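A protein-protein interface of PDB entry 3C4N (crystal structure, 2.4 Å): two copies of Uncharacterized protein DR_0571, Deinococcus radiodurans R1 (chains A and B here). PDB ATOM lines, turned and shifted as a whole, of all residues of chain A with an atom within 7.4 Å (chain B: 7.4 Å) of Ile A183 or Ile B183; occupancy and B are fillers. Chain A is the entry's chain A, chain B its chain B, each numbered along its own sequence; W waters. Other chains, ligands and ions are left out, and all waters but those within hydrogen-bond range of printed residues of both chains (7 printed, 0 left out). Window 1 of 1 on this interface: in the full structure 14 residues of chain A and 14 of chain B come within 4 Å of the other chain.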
ATOM      1  N   ALA A  52      27.581  -1.225 -11.594  1.00  0.00           N
ATOM      2  CA  ALA A  52      28.239  -2.432 -12.114  1.00  0.00           C
ATOM      3  C   ALA A  52      27.228  -3.287 -12.867  1.00  0.00           C
ATOM      4  O   ALA A  52      27.557  -3.902 -13.881  1.00  0.00           O
ATOM      5  CB  ALA A  52      28.871  -3.237 -10.983  1.00  0.00           C
ATOM      6  N   PHE A  53      25.995  -3.311 -12.373  1.00  0.00           N
ATOM      7  CA  PHE A  53      24.948  -4.074 -13.033  1.00  0.00           C
ATOM      8  C   PHE A  53      24.645  -3.478 -14.419  1.00  0.00           C
ATOM      9  O   PHE A  53      24.673  -4.192 -15.423  1.00  0.00           O
ATOM     10  CB  PHE A  53      23.686  -4.084 -12.176  1.00  0.00           C
ATOM     11  CG  PHE A  53      22.494  -4.638 -12.877  1.00  0.00           C
ATOM     12  CD1 PHE A  53      22.456  -5.968 -13.267  1.00  0.00           C
ATOM     13  CD2 PHE A  53      21.406  -3.825 -13.160  1.00  0.00           C
ATOM     14  CE1 PHE A  53      21.341  -6.489 -13.936  1.00  0.00           C
ATOM     15  CE2 PHE A  53      20.287  -4.327 -13.826  1.00  0.00           C
ATOM     16  CZ  PHE A  53      20.253  -5.664 -14.214  1.00  0.00           C
ATOM     17  N   ARG A  56      27.305  -4.115 -16.939  1.00  0.00           N
ATOM     18  CA  ARG A  56      27.367  -5.494 -17.428  1.00  0.00           C
ATOM     19  C   ARG A  56      26.366  -5.710 -18.550  1.00  0.00           C
ATOM     20  O   ARG A  56      26.573  -6.558 -19.417  1.00  0.00           O
ATOM     21  CB  ARG A  56      27.087  -6.512 -16.310  1.00  0.00           C
ATOM     22  CG  ARG A  56      28.150  -6.578 -15.211  1.00  0.00           C
ATOM     23  CD  ARG A  56      29.538  -6.776 -15.781  1.00  0.00           C
ATOM     24  NE  ARG A  56      29.644  -7.987 -16.586  1.00  0.00           N
ATOM     25  CZ  ARG A  56      30.670  -8.250 -17.389  1.00  0.00           C
ATOM     26  NH1 ARG A  56      31.670  -7.389 -17.496  1.00  0.00           N
ATOM     27  NH2 ARG A  56      30.706  -9.371 -18.089  1.00  0.00           N
ATOM     28  N   LEU A  66      34.558  -5.677  -9.533  1.00  0.00           N
ATOM     29  CA  LEU A  66      33.869  -4.990  -8.446  1.00  0.00           C
ATOM     30  C   LEU A  66      34.678  -5.193  -7.156  1.00  0.00           C
ATOM     31  O   LEU A  66      34.939  -6.335  -6.751  1.00  0.00           O
ATOM     32  CB  LEU A  66      32.452  -5.563  -8.265  1.00  0.00           C
ATOM     33  CG  LEU A  66      31.284  -4.630  -7.949  1.00  0.00           C
ATOM     34  CD1 LEU A  66      30.283  -5.351  -7.064  1.00  0.00           C
ATOM     35  CD2 LEU A  66      31.782  -3.366  -7.254  1.00  0.00           C
ATOM     36  N   LEU A  72      29.281  -8.804   1.219  1.00  0.00           N
ATOM     37  CA  LEU A  72      28.123  -8.626   0.362  1.00  0.00           C
ATOM     38  C   LEU A  72      26.917  -9.397   0.894  1.00  0.00           C
ATOM     39  O   LEU A  72      26.864 -10.618   0.804  1.00  0.00           O
ATOM     40  CB  LEU A  72      28.451  -9.114  -1.041  1.00  0.00           C
ATOM     41  CG  LEU A  72      27.374  -8.838  -2.079  1.00  0.00           C
ATOM     42  CD1 LEU A  72      27.360  -7.347  -2.407  1.00  0.00           C
ATOM     43  CD2 LEU A  72      27.657  -9.653  -3.316  1.00  0.00           C
ATOM     44  N   LYS A 114      13.679 -10.761 -11.505  1.00  0.00           N
ATOM     45  CA  LYS A 114      13.859 -11.119 -10.105  1.00  0.00           C
ATOM     46  C   LYS A 114      12.806 -10.470  -9.206  1.00  0.00           C
ATOM     47  O   LYS A 114      11.999  -9.645  -9.651  1.00  0.00           O
ATOM     48  CB  LYS A 114      15.264 -10.719  -9.632  1.00  0.00           C
ATOM     49  CG  LYS A 114      16.401 -11.562 -10.207  1.00  0.00           C
ATOM     50  CD  LYS A 114      16.284 -13.015  -9.771  1.00  0.00           C
ATOM     51  CE  LYS A 114      17.503 -13.856 -10.165  1.00  0.00           C
ATOM     52  NZ  LYS A 114      17.543 -14.242 -11.590  1.00  0.00           N
ATOM     53  N   LEU A 176      21.950  -5.710  -3.143  1.00  0.00           N
ATOM     54  CA  LEU A 176      22.300  -7.130  -3.245  1.00  0.00           C
ATOM     55  C   LEU A 176      21.857  -7.687  -4.598  1.00  0.00           C
ATOM     56  O   LEU A 176      22.620  -8.360  -5.290  1.00  0.00           O
ATOM     57  CB  LEU A 176      21.626  -7.939  -2.132  1.00  0.00           C
ATOM     58  CG  LEU A 176      22.011  -9.424  -2.127  1.00  0.00           C
ATOM     59  CD1 LEU A 176      23.508  -9.536  -1.908  1.00  0.00           C
ATOM     60  CD2 LEU A 176      21.246 -10.201  -1.043  1.00  0.00           C
ATOM     61  N   LEU A 177      20.607  -7.407  -4.954  1.00  0.00           N
ATOM     62  CA  LEU A 177      20.046  -7.856  -6.217  1.00  0.00           C
ATOM     63  C   LEU A 177      20.915  -7.392  -7.372  1.00  0.00           C
ATOM     64  O   LEU A 177      21.227  -8.156  -8.280  1.00  0.00           O
ATOM     65  CB  LEU A 177      18.638  -7.296  -6.411  1.00  0.00           C
ATOM     66  CG  LEU A 177      18.060  -7.410  -7.820  1.00  0.00           C
ATOM     67  CD1 LEU A 177      17.980  -8.865  -8.258  1.00  0.00           C
ATOM     68  CD2 LEU A 177      16.691  -6.786  -7.831  1.00  0.00           C
ATOM     69  N   ALA A 178      21.306  -6.128  -7.331  1.00  0.00           N
ATOM     70  CA  ALA A 178      22.117  -5.566  -8.387  1.00  0.00           C
ATOM     71  C   ALA A 178      23.469  -6.248  -8.418  1.00  0.00           C
ATOM     72  O   ALA A 178      23.953  -6.623  -9.483  1.00  0.00           O
ATOM     73  CB  ALA A 178      22.279  -4.070  -8.181  1.00  0.00           C
ATOM     74  N   ALA A 179      24.086  -6.423  -7.258  1.00  0.00           N
ATOM     75  CA  ALA A 179      25.389  -7.078  -7.234  1.00  0.00           C
ATOM     76  C   ALA A 179      25.236  -8.510  -7.760  1.00  0.00           C
ATOM     77  O   ALA A 179      25.969  -8.930  -8.647  1.00  0.00           O
ATOM     78  CB  ALA A 179      25.962  -7.081  -5.817  1.00  0.00           C
ATOM     79  N   GLN A 180      24.271  -9.248  -7.225  1.00  0.00           N
ATOM     80  CA  GLN A 180      24.059 -10.616  -7.661  1.00  0.00           C
ATOM     81  C   GLN A 180      23.974 -10.744  -9.175  1.00  0.00           C
ATOM     82  O   GLN A 180      24.729 -11.508  -9.789  1.00  0.00           O
ATOM     83  CB  GLN A 180      22.801 -11.184  -7.011  1.00  0.00           C
ATOM     84  CG  GLN A 180      23.008 -11.417  -5.539  1.00  0.00           C
ATOM     85  CD  GLN A 180      21.823 -12.046  -4.878  1.00  0.00           C
ATOM     86  OE1 GLN A 180      20.675 -11.750  -5.231  1.00  0.00           O
ATOM     87  NE2 GLN A 180      22.082 -12.916  -3.897  1.00  0.00           N
ATOM     88  N   GLN A 181      23.061  -9.981  -9.766  1.00  0.00           N
ATOM     89  CA  GLN A 181      22.849  -9.960 -11.204  1.00  0.00           C
ATOM     90  C   GLN A 181      24.125  -9.573 -11.953  1.00  0.00           C
ATOM     91  O   GLN A 181      24.399 -10.109 -13.024  1.00  0.00           O
ATOM     92  CB  GLN A 181      21.724  -8.974 -11.554  1.00  0.00           C
ATOM     93  CG  GLN A 181      20.311  -9.455 -11.242  1.00  0.00           C
ATOM     94  CD  GLN A 181      20.033 -10.842 -11.798  1.00  0.00           C
ATOM     95  OE1 GLN A 181      20.266 -11.841 -11.118  1.00  0.00           O
ATOM     96  NE2 GLN A 181      19.546 -10.911 -13.036  1.00  0.00           N
ATOM     97  N   ALA A 182      24.900  -8.639 -11.399  1.00  0.00           N
ATOM     98  CA  ALA A 182      26.146  -8.207 -12.039  1.00  0.00           C
ATOM     99  C   ALA A 182      27.145  -9.363 -12.064  1.00  0.00           C
ATOM    100  O   ALA A 182      27.859  -9.577 -13.056  1.00  0.00           O
ATOM    101  CB  ALA A 182      26.737  -7.018 -11.287  1.00  0.00           C
ATOM    102  N   ILE A 183      27.186 -10.097 -10.954  1.00  0.00           N
ATOM    103  CA  ILE A 183      28.070 -11.251 -10.800  1.00  0.00           C
ATOM    104  C   ILE A 183      27.633 -12.380 -11.721  1.00  0.00           C
ATOM    105  O   ILE A 183      28.465 -13.077 -12.306  1.00  0.00           O
ATOM    106  CB  ILE A 183      28.056 -11.788  -9.359  1.00  0.00           C
ATOM    107  CG1 ILE A 183      28.693 -10.764  -8.406  1.00  0.00           C
ATOM    108  CG2 ILE A 183      28.773 -13.105  -9.314  1.00  0.00           C
ATOM    109  CD1 ILE A 183      28.329 -10.967  -6.934  1.00  0.00           C
ATOM    110  N   GLY A 184      26.320 -12.558 -11.840  1.00  0.00           N
ATOM    111  CA  GLY A 184      25.797 -13.597 -12.708  1.00  0.00           C
ATOM    112  C   GLY A 184      26.019 -13.211 -14.152  1.00  0.00           C
ATOM    113  O   GLY A 184      25.750 -13.995 -15.055  1.00  0.00           O
ATOM    114  N   GLN A 185      26.496 -11.988 -14.365  1.00  0.00           N
ATOM    115  CA  GLN A 185      26.752 -11.530 -15.715  1.00  0.00           C
ATOM    116  C   GLN A 185      28.232 -11.449 -16.004  1.00  0.00           C
ATOM    117  O   GLN A 185      28.650 -10.799 -16.960  1.00  0.00           O
ATOM    118  CB  GLN A 185      26.094 -10.180 -15.969  1.00  0.00           C
ATOM    119  CG  GLN A 185      24.597 -10.212 -15.824  1.00  0.00           C
ATOM    120  CD  GLN A 185      23.957 -11.212 -16.742  1.00  0.00           C
ATOM    121  OE1 GLN A 185      24.040 -11.078 -17.964  1.00  0.00           O
ATOM    122  NE2 GLN A 185      23.313 -12.231 -16.167  1.00  0.00           N
ATOM    123  N   GLY A 186      29.028 -12.110 -15.175  1.00  0.00           N
ATOM    124  CA  GLY A 186      30.464 -12.127 -15.401  1.00  0.00           C
ATOM    125  C   GLY A 186      31.263 -10.982 -14.816  1.00  0.00           C
ATOM    126  O   GLY A 186      32.367 -10.671 -15.275  1.00  0.00           O
ATOM    127  N   ALA A 187      30.709 -10.338 -13.805  1.00  0.00           N
ATOM    128  CA  ALA A 187      31.425  -9.243 -13.170  1.00  0.00           C
ATOM    129  C   ALA A 187      32.425  -9.850 -12.194  1.00  0.00           C
ATOM    130  O   ALA A 187      32.068 -10.734 -11.410  1.00  0.00           O
ATOM    131  CB  ALA A 187      30.454  -8.331 -12.425  1.00  0.00           C
ATOM    132  N   GLY A 188      33.672  -9.401 -12.261  1.00  0.00           N
ATOM    133  CA  GLY A 188      34.664  -9.910 -11.342  1.00  0.00           C
ATOM    134  C   GLY A 188      34.245  -9.426  -9.970  1.00  0.00           C
ATOM    135  O   GLY A 188      33.653  -8.354  -9.857  1.00  0.00           O
ATOM    136  N   LEU A 189      34.526 -10.193  -8.926  1.00  0.00           N
ATOM    137  CA  LEU A 189      34.140  -9.777  -7.589  1.00  0.00           C
ATOM    138  C   LEU A 189      35.279  -9.912  -6.604  1.00  0.00           C
ATOM    139  O   LEU A 189      35.934 -10.947  -6.521  1.00  0.00           O
ATOM    140  CB  LEU A 189      32.942 -10.596  -7.109  1.00  0.00           C
ATOM    141  CG  LEU A 189      32.257 -10.270  -5.766  1.00  0.00           C
ATOM    142  CD1 LEU A 189      33.072 -10.795  -4.604  1.00  0.00           C
ATOM    143  CD2 LEU A 189      32.023  -8.780  -5.651  1.00  0.00           C
ATOM    144  N   LEU A 191      35.882  -9.015  -2.538  1.00  0.00           N
ATOM    145  CA  LEU A 191      35.335  -8.522  -1.284  1.00  0.00           C
ATOM    146  C   LEU A 191      36.442  -8.370  -0.253  1.00  0.00           C
ATOM    147  O   LEU A 191      37.590  -8.735  -0.509  1.00  0.00           O
ATOM    148  CB  LEU A 191      34.272  -9.484  -0.755  1.00  0.00           C
ATOM    149  CG  LEU A 191      33.107  -9.760  -1.701  1.00  0.00           C
ATOM    150  CD1 LEU A 191      32.231 -10.866  -1.133  1.00  0.00           C
ATOM    151  CD2 LEU A 191      32.294  -8.494  -1.911  1.00  0.00           C
ATOM    152  N   ALA B  52      26.240 -25.865  -5.125  1.00  0.00           N
ATOM    153  CA  ALA B  52      25.443 -24.688  -4.760  1.00  0.00           C
ATOM    154  C   ALA B  52      24.595 -24.244  -5.949  1.00  0.00           C
ATOM    155  O   ALA B  52      23.455 -23.808  -5.789  1.00  0.00           O
ATOM    156  CB  ALA B  52      26.340 -23.553  -4.301  1.00  0.00           C
ATOM    157  N   PHE B  53      25.152 -24.368  -7.149  1.00  0.00           N
ATOM    158  CA  PHE B  53      24.420 -24.007  -8.347  1.00  0.00           C
ATOM    159  C   PHE B  53      23.212 -24.936  -8.539  1.00  0.00           C
ATOM    160  O   PHE B  53      22.087 -24.468  -8.688  1.00  0.00           O
ATOM    161  CB  PHE B  53      25.337 -24.081  -9.566  1.00  0.00           C
ATOM    162  CG  PHE B  53      24.616 -23.943 -10.865  1.00  0.00           C
ATOM    163  CD1 PHE B  53      23.962 -22.764 -11.193  1.00  0.00           C
ATOM    164  CD2 PHE B  53      24.575 -25.001 -11.757  1.00  0.00           C
ATOM    165  CE1 PHE B  53      23.271 -22.638 -12.404  1.00  0.00           C
ATOM    166  CE2 PHE B  53      23.891 -24.891 -12.967  1.00  0.00           C
ATOM    167  CZ  PHE B  53      23.238 -23.707 -13.291  1.00  0.00           C
ATOM    168  N   ARG B  56      20.450 -24.317  -6.117  1.00  0.00           N
ATOM    169  CA  ARG B  56      19.684 -23.091  -6.363  1.00  0.00           C
ATOM    170  C   ARG B  56      18.604 -23.332  -7.408  1.00  0.00           C
ATOM    171  O   ARG B  56      17.568 -22.671  -7.397  1.00  0.00           O
ATOM    172  CB  ARG B  56      20.586 -21.940  -6.835  1.00  0.00           C
ATOM    173  CG  ARG B  56      21.577 -21.422  -5.793  1.00  0.00           C
ATOM    174  CD  ARG B  56      20.899 -21.053  -4.488  1.00  0.00           C
ATOM    175  NE  ARG B  56      19.862 -20.048  -4.663  1.00  0.00           N
ATOM    176  CZ  ARG B  56      18.948 -19.769  -3.743  1.00  0.00           C
ATOM    177  NH1 ARG B  56      18.945 -20.422  -2.590  1.00  0.00           N
ATOM    178  NH2 ARG B  56      18.036 -18.841  -3.967  1.00  0.00           N
ATOM    179  N   LEU B  66      26.897 -19.715   0.764  1.00  0.00           N
ATOM    180  CA  LEU B  66      28.146 -20.279   0.259  1.00  0.00           C
ATOM    181  C   LEU B  66      29.316 -19.650   1.020  1.00  0.00           C
ATOM    182  O   LEU B  66      29.473 -18.420   1.023  1.00  0.00           O
ATOM    183  CB  LEU B  66      28.297 -19.993  -1.248  1.00  0.00           C
ATOM    184  CG  LEU B  66      28.869 -21.063  -2.173  1.00  0.00           C
ATOM    185  CD1 LEU B  66      29.645 -20.395  -3.294  1.00  0.00           C
ATOM    186  CD2 LEU B  66      29.772 -22.010  -1.403  1.00  0.00           C
ATOM    187  N   LEU B  72      37.091 -15.521  -4.874  1.00  0.00           N
ATOM    188  CA  LEU B  72      36.359 -16.111  -5.979  1.00  0.00           C
ATOM    189  C   LEU B  72      36.792 -15.512  -7.311  1.00  0.00           C
ATOM    190  O   LEU B  72      36.451 -14.376  -7.626  1.00  0.00           O
ATOM    191  CB  LEU B  72      34.871 -15.876  -5.790  1.00  0.00           C
ATOM    192  CG  LEU B  72      33.985 -16.586  -6.804  1.00  0.00           C
ATOM    193  CD1 LEU B  72      33.977 -18.083  -6.497  1.00  0.00           C
ATOM    194  CD2 LEU B  72      32.588 -16.014  -6.728  1.00  0.00           C
ATOM    195  N   LYS B 114      25.265 -19.618 -20.762  1.00  0.00           N
ATOM    196  CA  LYS B 114      26.542 -18.931 -20.632  1.00  0.00           C
ATOM    197  C   LYS B 114      27.619 -19.574 -21.500  1.00  0.00           C
ATOM    198  O   LYS B 114      27.404 -20.621 -22.113  1.00  0.00           O
ATOM    199  CB  LYS B 114      26.993 -18.921 -19.164  1.00  0.00           C
ATOM    200  CG  LYS B 114      26.177 -18.011 -18.245  1.00  0.00           C
ATOM    201  CD  LYS B 114      26.319 -16.559 -18.664  1.00  0.00           C
ATOM    202  CE  LYS B 114      25.674 -15.591 -17.674  1.00  0.00           C
ATOM    203  NZ  LYS B 114      24.206 -15.524 -17.767  1.00  0.00           N
ATOM    204  N   LEU B 176      33.936 -20.927 -11.448  1.00  0.00           N
ATOM    205  CA  LEU B 176      33.525 -19.525 -11.405  1.00  0.00           C
ATOM    206  C   LEU B 176      32.116 -19.377 -11.974  1.00  0.00           C
ATOM    207  O   LEU B 176      31.261 -18.728 -11.378  1.00  0.00           O
ATOM    208  CB  LEU B 176      34.481 -18.651 -12.223  1.00  0.00           C
ATOM    209  CG  LEU B 176      34.145 -17.154 -12.167  1.00  0.00           C
ATOM    210  CD1 LEU B 176      34.243 -16.694 -10.727  1.00  0.00           C
ATOM    211  CD2 LEU B 176      35.088 -16.325 -13.059  1.00  0.00           C
ATOM    212  N   LEU B 177      31.896 -19.985 -13.136  1.00  0.00           N
ATOM    213  CA  LEU B 177      30.611 -19.940 -13.813  1.00  0.00           C
ATOM    214  C   LEU B 177      29.524 -20.452 -12.897  1.00  0.00           C
ATOM    215  O   LEU B 177      28.453 -19.858 -12.793  1.00  0.00           O
ATOM    216  CB  LEU B 177      30.634 -20.800 -15.073  1.00  0.00           C
ATOM    217  CG  LEU B 177      29.270 -21.112 -15.682  1.00  0.00           C
ATOM    218  CD1 LEU B 177      28.543 -19.826 -16.072  1.00  0.00           C
ATOM    219  CD2 LEU B 177      29.469 -21.992 -16.887  1.00  0.00           C
ATOM    220  N   ALA B 178      29.807 -21.560 -12.232  1.00  0.00           N
ATOM    221  CA  ALA B 178      28.833 -22.158 -11.338  1.00  0.00           C
ATOM    222  C   ALA B 178      28.573 -21.230 -10.168  1.00  0.00           C
ATOM    223  O   ALA B 178      27.425 -20.995  -9.798  1.00  0.00           O
ATOM    224  CB  ALA B 178      29.333 -23.508 -10.849  1.00  0.00           C
ATOM    225  N   ALA B 179      29.632 -20.692  -9.580  1.00  0.00           N
ATOM    226  CA  ALA B 179      29.440 -19.790  -8.455  1.00  0.00           C
ATOM    227  C   ALA B 179      28.637 -18.568  -8.923  1.00  0.00           C
ATOM    228  O   ALA B 179      27.639 -18.207  -8.314  1.00  0.00           O
ATOM    229  CB  ALA B 179      30.782 -19.361  -7.876  1.00  0.00           C
ATOM    230  N   GLN B 180      29.068 -17.942 -10.010  1.00  0.00           N
ATOM    231  CA  GLN B 180      28.374 -16.777 -10.519  1.00  0.00           C
ATOM    232  C   GLN B 180      26.877 -17.003 -10.658  1.00  0.00           C
ATOM    233  O   GLN B 180      26.067 -16.253 -10.102  1.00  0.00           O
ATOM    234  CB  GLN B 180      28.972 -16.357 -11.855  1.00  0.00           C
ATOM    235  CG  GLN B 180      30.348 -15.770 -11.675  1.00  0.00           C
ATOM    236  CD  GLN B 180      30.943 -15.272 -12.955  1.00  0.00           C
ATOM    237  OE1 GLN B 180      30.733 -15.861 -14.020  1.00  0.00           O
ATOM    238  NE2 GLN B 180      31.707 -14.186 -12.868  1.00  0.00           N
ATOM    239  N   GLN B 181      26.520 -18.050 -11.395  1.00  0.00           N
ATOM    240  CA  GLN B 181      25.135 -18.423 -11.625  1.00  0.00           C
ATOM    241  C   GLN B 181      24.395 -18.691 -10.307  1.00  0.00           C
ATOM    242  O   GLN B 181      23.217 -18.352 -10.173  1.00  0.00           O
ATOM    243  CB  GLN B 181      25.070 -19.673 -12.516  1.00  0.00           C
ATOM    244  CG  GLN B 181      25.350 -19.439 -13.995  1.00  0.00           C
ATOM    245  CD  GLN B 181      24.539 -18.288 -14.566  1.00  0.00           C
ATOM    246  OE1 GLN B 181      24.981 -17.140 -14.550  1.00  0.00           O
ATOM    247  NE2 GLN B 181      23.345 -18.589 -15.060  1.00  0.00           N
ATOM    248  N   ALA B 182      25.078 -19.300  -9.338  1.00  0.00           N
ATOM    249  CA  ALA B 182      24.462 -19.595  -8.045  1.00  0.00           C
ATOM    250  C   ALA B 182      24.143 -18.291  -7.317  1.00  0.00           C
ATOM    251  O   ALA B 182      23.091 -18.150  -6.675  1.00  0.00           O
ATOM    252  CB  ALA B 182      25.390 -20.450  -7.199  1.00  0.00           C
ATOM    253  N   ILE B 183      25.071 -17.343  -7.422  1.00  0.00           N
ATOM    254  CA  ILE B 183      24.923 -16.022  -6.805  1.00  0.00           C
ATOM    255  C   ILE B 183      23.817 -15.235  -7.497  1.00  0.00           C
ATOM    256  O   ILE B 183      23.045 -14.522  -6.849  1.00  0.00           O
ATOM    257  CB  ILE B 183      26.217 -15.198  -6.906  1.00  0.00           C
ATOM    258  CG1 ILE B 183      27.316 -15.834  -6.043  1.00  0.00           C
ATOM    259  CG2 ILE B 183      25.933 -13.789  -6.490  1.00  0.00           C
ATOM    260  CD1 ILE B 183      28.733 -15.390  -6.414  1.00  0.00           C
ATOM    261  N   GLY B 184      23.753 -15.361  -8.819  1.00  0.00           N
ATOM    262  CA  GLY B 184      22.723 -14.672  -9.573  1.00  0.00           C
ATOM    263  C   GLY B 184      21.378 -15.306  -9.284  1.00  0.00           C
ATOM    264  O   GLY B 184      20.342 -14.800  -9.708  1.00  0.00           O
ATOM    265  N   GLN B 185      21.396 -16.425  -8.565  1.00  0.00           N
ATOM    266  CA  GLN B 185      20.160 -17.097  -8.237  1.00  0.00           C
ATOM    267  C   GLN B 185      19.793 -16.926  -6.783  1.00  0.00           C
ATOM    268  O   GLN B 185      18.957 -17.658  -6.252  1.00  0.00           O
ATOM    269  CB  GLN B 185      20.232 -18.577  -8.593  1.00  0.00           C
ATOM    270  CG  GLN B 185      20.460 -18.819 -10.066  1.00  0.00           C
ATOM    271  CD  GLN B 185      19.388 -18.188 -10.922  1.00  0.00           C
ATOM    272  OE1 GLN B 185      18.212 -18.560 -10.828  1.00  0.00           O
ATOM    273  NE2 GLN B 185      19.779 -17.224 -11.763  1.00  0.00           N
ATOM    274  N   GLY B 186      20.417 -15.951  -6.137  1.00  0.00           N
ATOM    275  CA  GLY B 186      20.101 -15.680  -4.743  1.00  0.00           C
ATOM    276  C   GLY B 186      20.858 -16.475  -3.699  1.00  0.00           C
ATOM    277  O   GLY B 186      20.410 -16.621  -2.557  1.00  0.00           O
ATOM    278  N   ALA B 187      22.007 -17.002  -4.084  1.00  0.00           N
ATOM    279  CA  ALA B 187      22.811 -17.760  -3.139  1.00  0.00           C
ATOM    280  C   ALA B 187      23.580 -16.769  -2.275  1.00  0.00           C
ATOM    281  O   ALA B 187      24.200 -15.840  -2.797  1.00  0.00           O
ATOM    282  CB  ALA B 187      23.780 -18.662  -3.878  1.00  0.00           C
ATOM    283  N   GLY B 188      23.513 -16.947  -0.961  1.00  0.00           N
ATOM    284  CA  GLY B 188      24.244 -16.062  -0.079  1.00  0.00           C
ATOM    285  C   GLY B 188      25.711 -16.310  -0.364  1.00  0.00           C
ATOM    286  O   GLY B 188      26.081 -17.426  -0.721  1.00  0.00           O
ATOM    287  N   LEU B 189      26.551 -15.297  -0.225  1.00  0.00           N
ATOM    288  CA  LEU B 189      27.968 -15.486  -0.495  1.00  0.00           C
ATOM    289  C   LEU B 189      28.832 -14.908   0.607  1.00  0.00           C
ATOM    290  O   LEU B 189      28.660 -13.764   1.022  1.00  0.00           O
ATOM    291  CB  LEU B 189      28.345 -14.844  -1.833  1.00  0.00           C
ATOM    292  CG  LEU B 189      29.767 -15.006  -2.405  1.00  0.00           C
ATOM    293  CD1 LEU B 189      30.736 -14.096  -1.694  1.00  0.00           C
ATOM    294  CD2 LEU B 189      30.197 -16.452  -2.310  1.00  0.00           C
ATOM    295  N   LEU B 191      32.945 -14.765   1.454  1.00  0.00           N
ATOM    296  CA  LEU B 191      34.307 -15.077   1.056  1.00  0.00           C
ATOM    297  C   LEU B 191      35.275 -14.772   2.194  1.00  0.00           C
ATOM    298  O   LEU B 191      34.877 -14.243   3.236  1.00  0.00           O
ATOM    299  CB  LEU B 191      34.687 -14.261  -0.176  1.00  0.00           C
ATOM    300  CG  LEU B 191      33.781 -14.444  -1.393  1.00  0.00           C
ATOM    301  CD1 LEU B 191      34.171 -13.457  -2.482  1.00  0.00           C
ATOM    302  CD2 LEU B 191      33.888 -15.872  -1.901  1.00  0.00           C
HETATM  303  O   HOH W   1      32.496 -13.113  -9.951  1.00  0.00           O
HETATM  304  O   HOH W   2      25.000 -12.983  -2.910  1.00  0.00           O
HETATM  305  O   HOH W   3      25.600 -12.501  -0.066  1.00  0.00           O
HETATM  306  O   HOH W   4      22.962 -14.024 -19.338  1.00  0.00           O
HETATM  307  O   HOH W   5      29.738 -11.190   2.022  1.00  0.00           O
HETATM  308  O   HOH W   6      35.347 -12.937  -9.199  1.00  0.00           O
HETATM  309  O   HOH W   7      37.250 -12.991  -4.604  1.00  0.00           O
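Of the 21 printed residues of chain B, 11 touch a printed residue of chain A. Among the printed residues, 20 pairs touch across the chains.
Ile A183 touches just these residues of chain B: Gln B180 (3.3 Å) and Ile B183 (3.7 Å). Of the printed residues of chain B, Leu A191 touches Leu B189 (3.6 Å) and Leu B191 (3.5 Å). Of the printed residues of chain A, Leu B72 touches Leu A189 (3.6 Å). Of the printed residues of chain A, Lys B114 touches Gly A184 and Gln A185. Ala B182 touches none of the printed residues of chain A. Of chain A, only Gln A180 (3.4 Å) and Ile A183 (3.7 Å) come within 4 Å of Ile B183. Printed residues of chain A within 4 Å of Ala B187: Gln A180 (3.8 Å). The nearest printed residue of chain B that does not touch Leu A72 is Ile B183 (5.5 Å).
Gln A180 touches Gly B184, and with the chains exchanged Gly A184 touches Gln B180. Gln A180 touches Ala B187, and with the chains exchanged Ala A187 touches Gln B180. Ile A183 touches its own counterpart, Ile B183. Leu A191 touches its own counterpart, Leu B191. Positions printed for both chains: 52, 53, 56, 66, 72, 114, 176, 177, 178, 179, 180, 181, 182, 183, 184, 185, 186, 187, 188, 189 and 191. Of the 20 pairs that touch across the chains among the printed residues, 20 have their exchanged pair printed and touching as well.
Water W6 bridges O of Leu B72 and N of Leu A189. Water W3 bridges O of Leu A72 (2.4 Å) and N of Leu B189 (3.0 Å). Water W4 lies within hydrogen-bond range of the side-chain amino group (NZ) of Lys B114 and the side-chain amide oxygen (OE1) of Gln A185. Water W5 lies within hydrogen-bond range of the backbone NH (N) of Leu A72 (2.6 Å) and the backbone carbonyl oxygen (O) of Leu B189 (3.0 Å). Water W1 bridges O of Ala A187 and NE2 of Gln B180. Water W2 lies within hydrogen-bond range of the backbone carbonyl oxygen of Ala B187 (3.0 Å) and the side-chain amide nitrogen of Gln A180 (3.1 Å).
NE2 of Gln A180 lies close to O of Ile B183 (3.5 Å). OE1 of Gln A181 lies close to O of Gly B184, at 3.3 Å. O of Gly A184 lies close to NZ of Lys B114 (3.5 Å). The backbone carbonyl oxygen (O) of Gly B184 lies close to the side-chain amino group (NZ) of Lys A114 (3.4 Å). OE1 of Gln B181 sits close to O of Gly A184 (3.3 Å). O of Ile A183 lies close to NE2 of Gln B180 (3.5 Å).
N of Ala A187 lies close to O of Ala A182. O of Gln B185 is in hydrogen-bond range of NH2 of Arg B56, 2.7 Å away. The backbone NH of Ala B187 lies close to the backbone carbonyl oxygen of Ala B182, at 3.0 Å. The guanidinium group of Arg A56 sits at hydrogen-bond distance from the backbone carbonyl oxygen of Gln A185, 2.7 Å away.
O of Leu A72 touches O of Leu B189, at 3.6 Å. Lys A114 touches Gln B185 (NZ to NE2, 3.7 Å). Gly B186 touches Gln A180 (CA to NE2, 3.5 Å). Gln A180 touches Ala B187 (NE2 to O, 3.8 Å). Ile B183 touches Ile A183 (CD1 to CG2, 3.7 Å). Gln B180 touches Gly A186 (NE2 to CA, 3.5 Å). O of Ala A187 touches NE2 of Gln B180, at 3.8 Å. Leu A189 touches Leu B72 (O to O, 3.6 Å). Leu B191 touches Leu A189. Leu A191 touches Leu B191.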
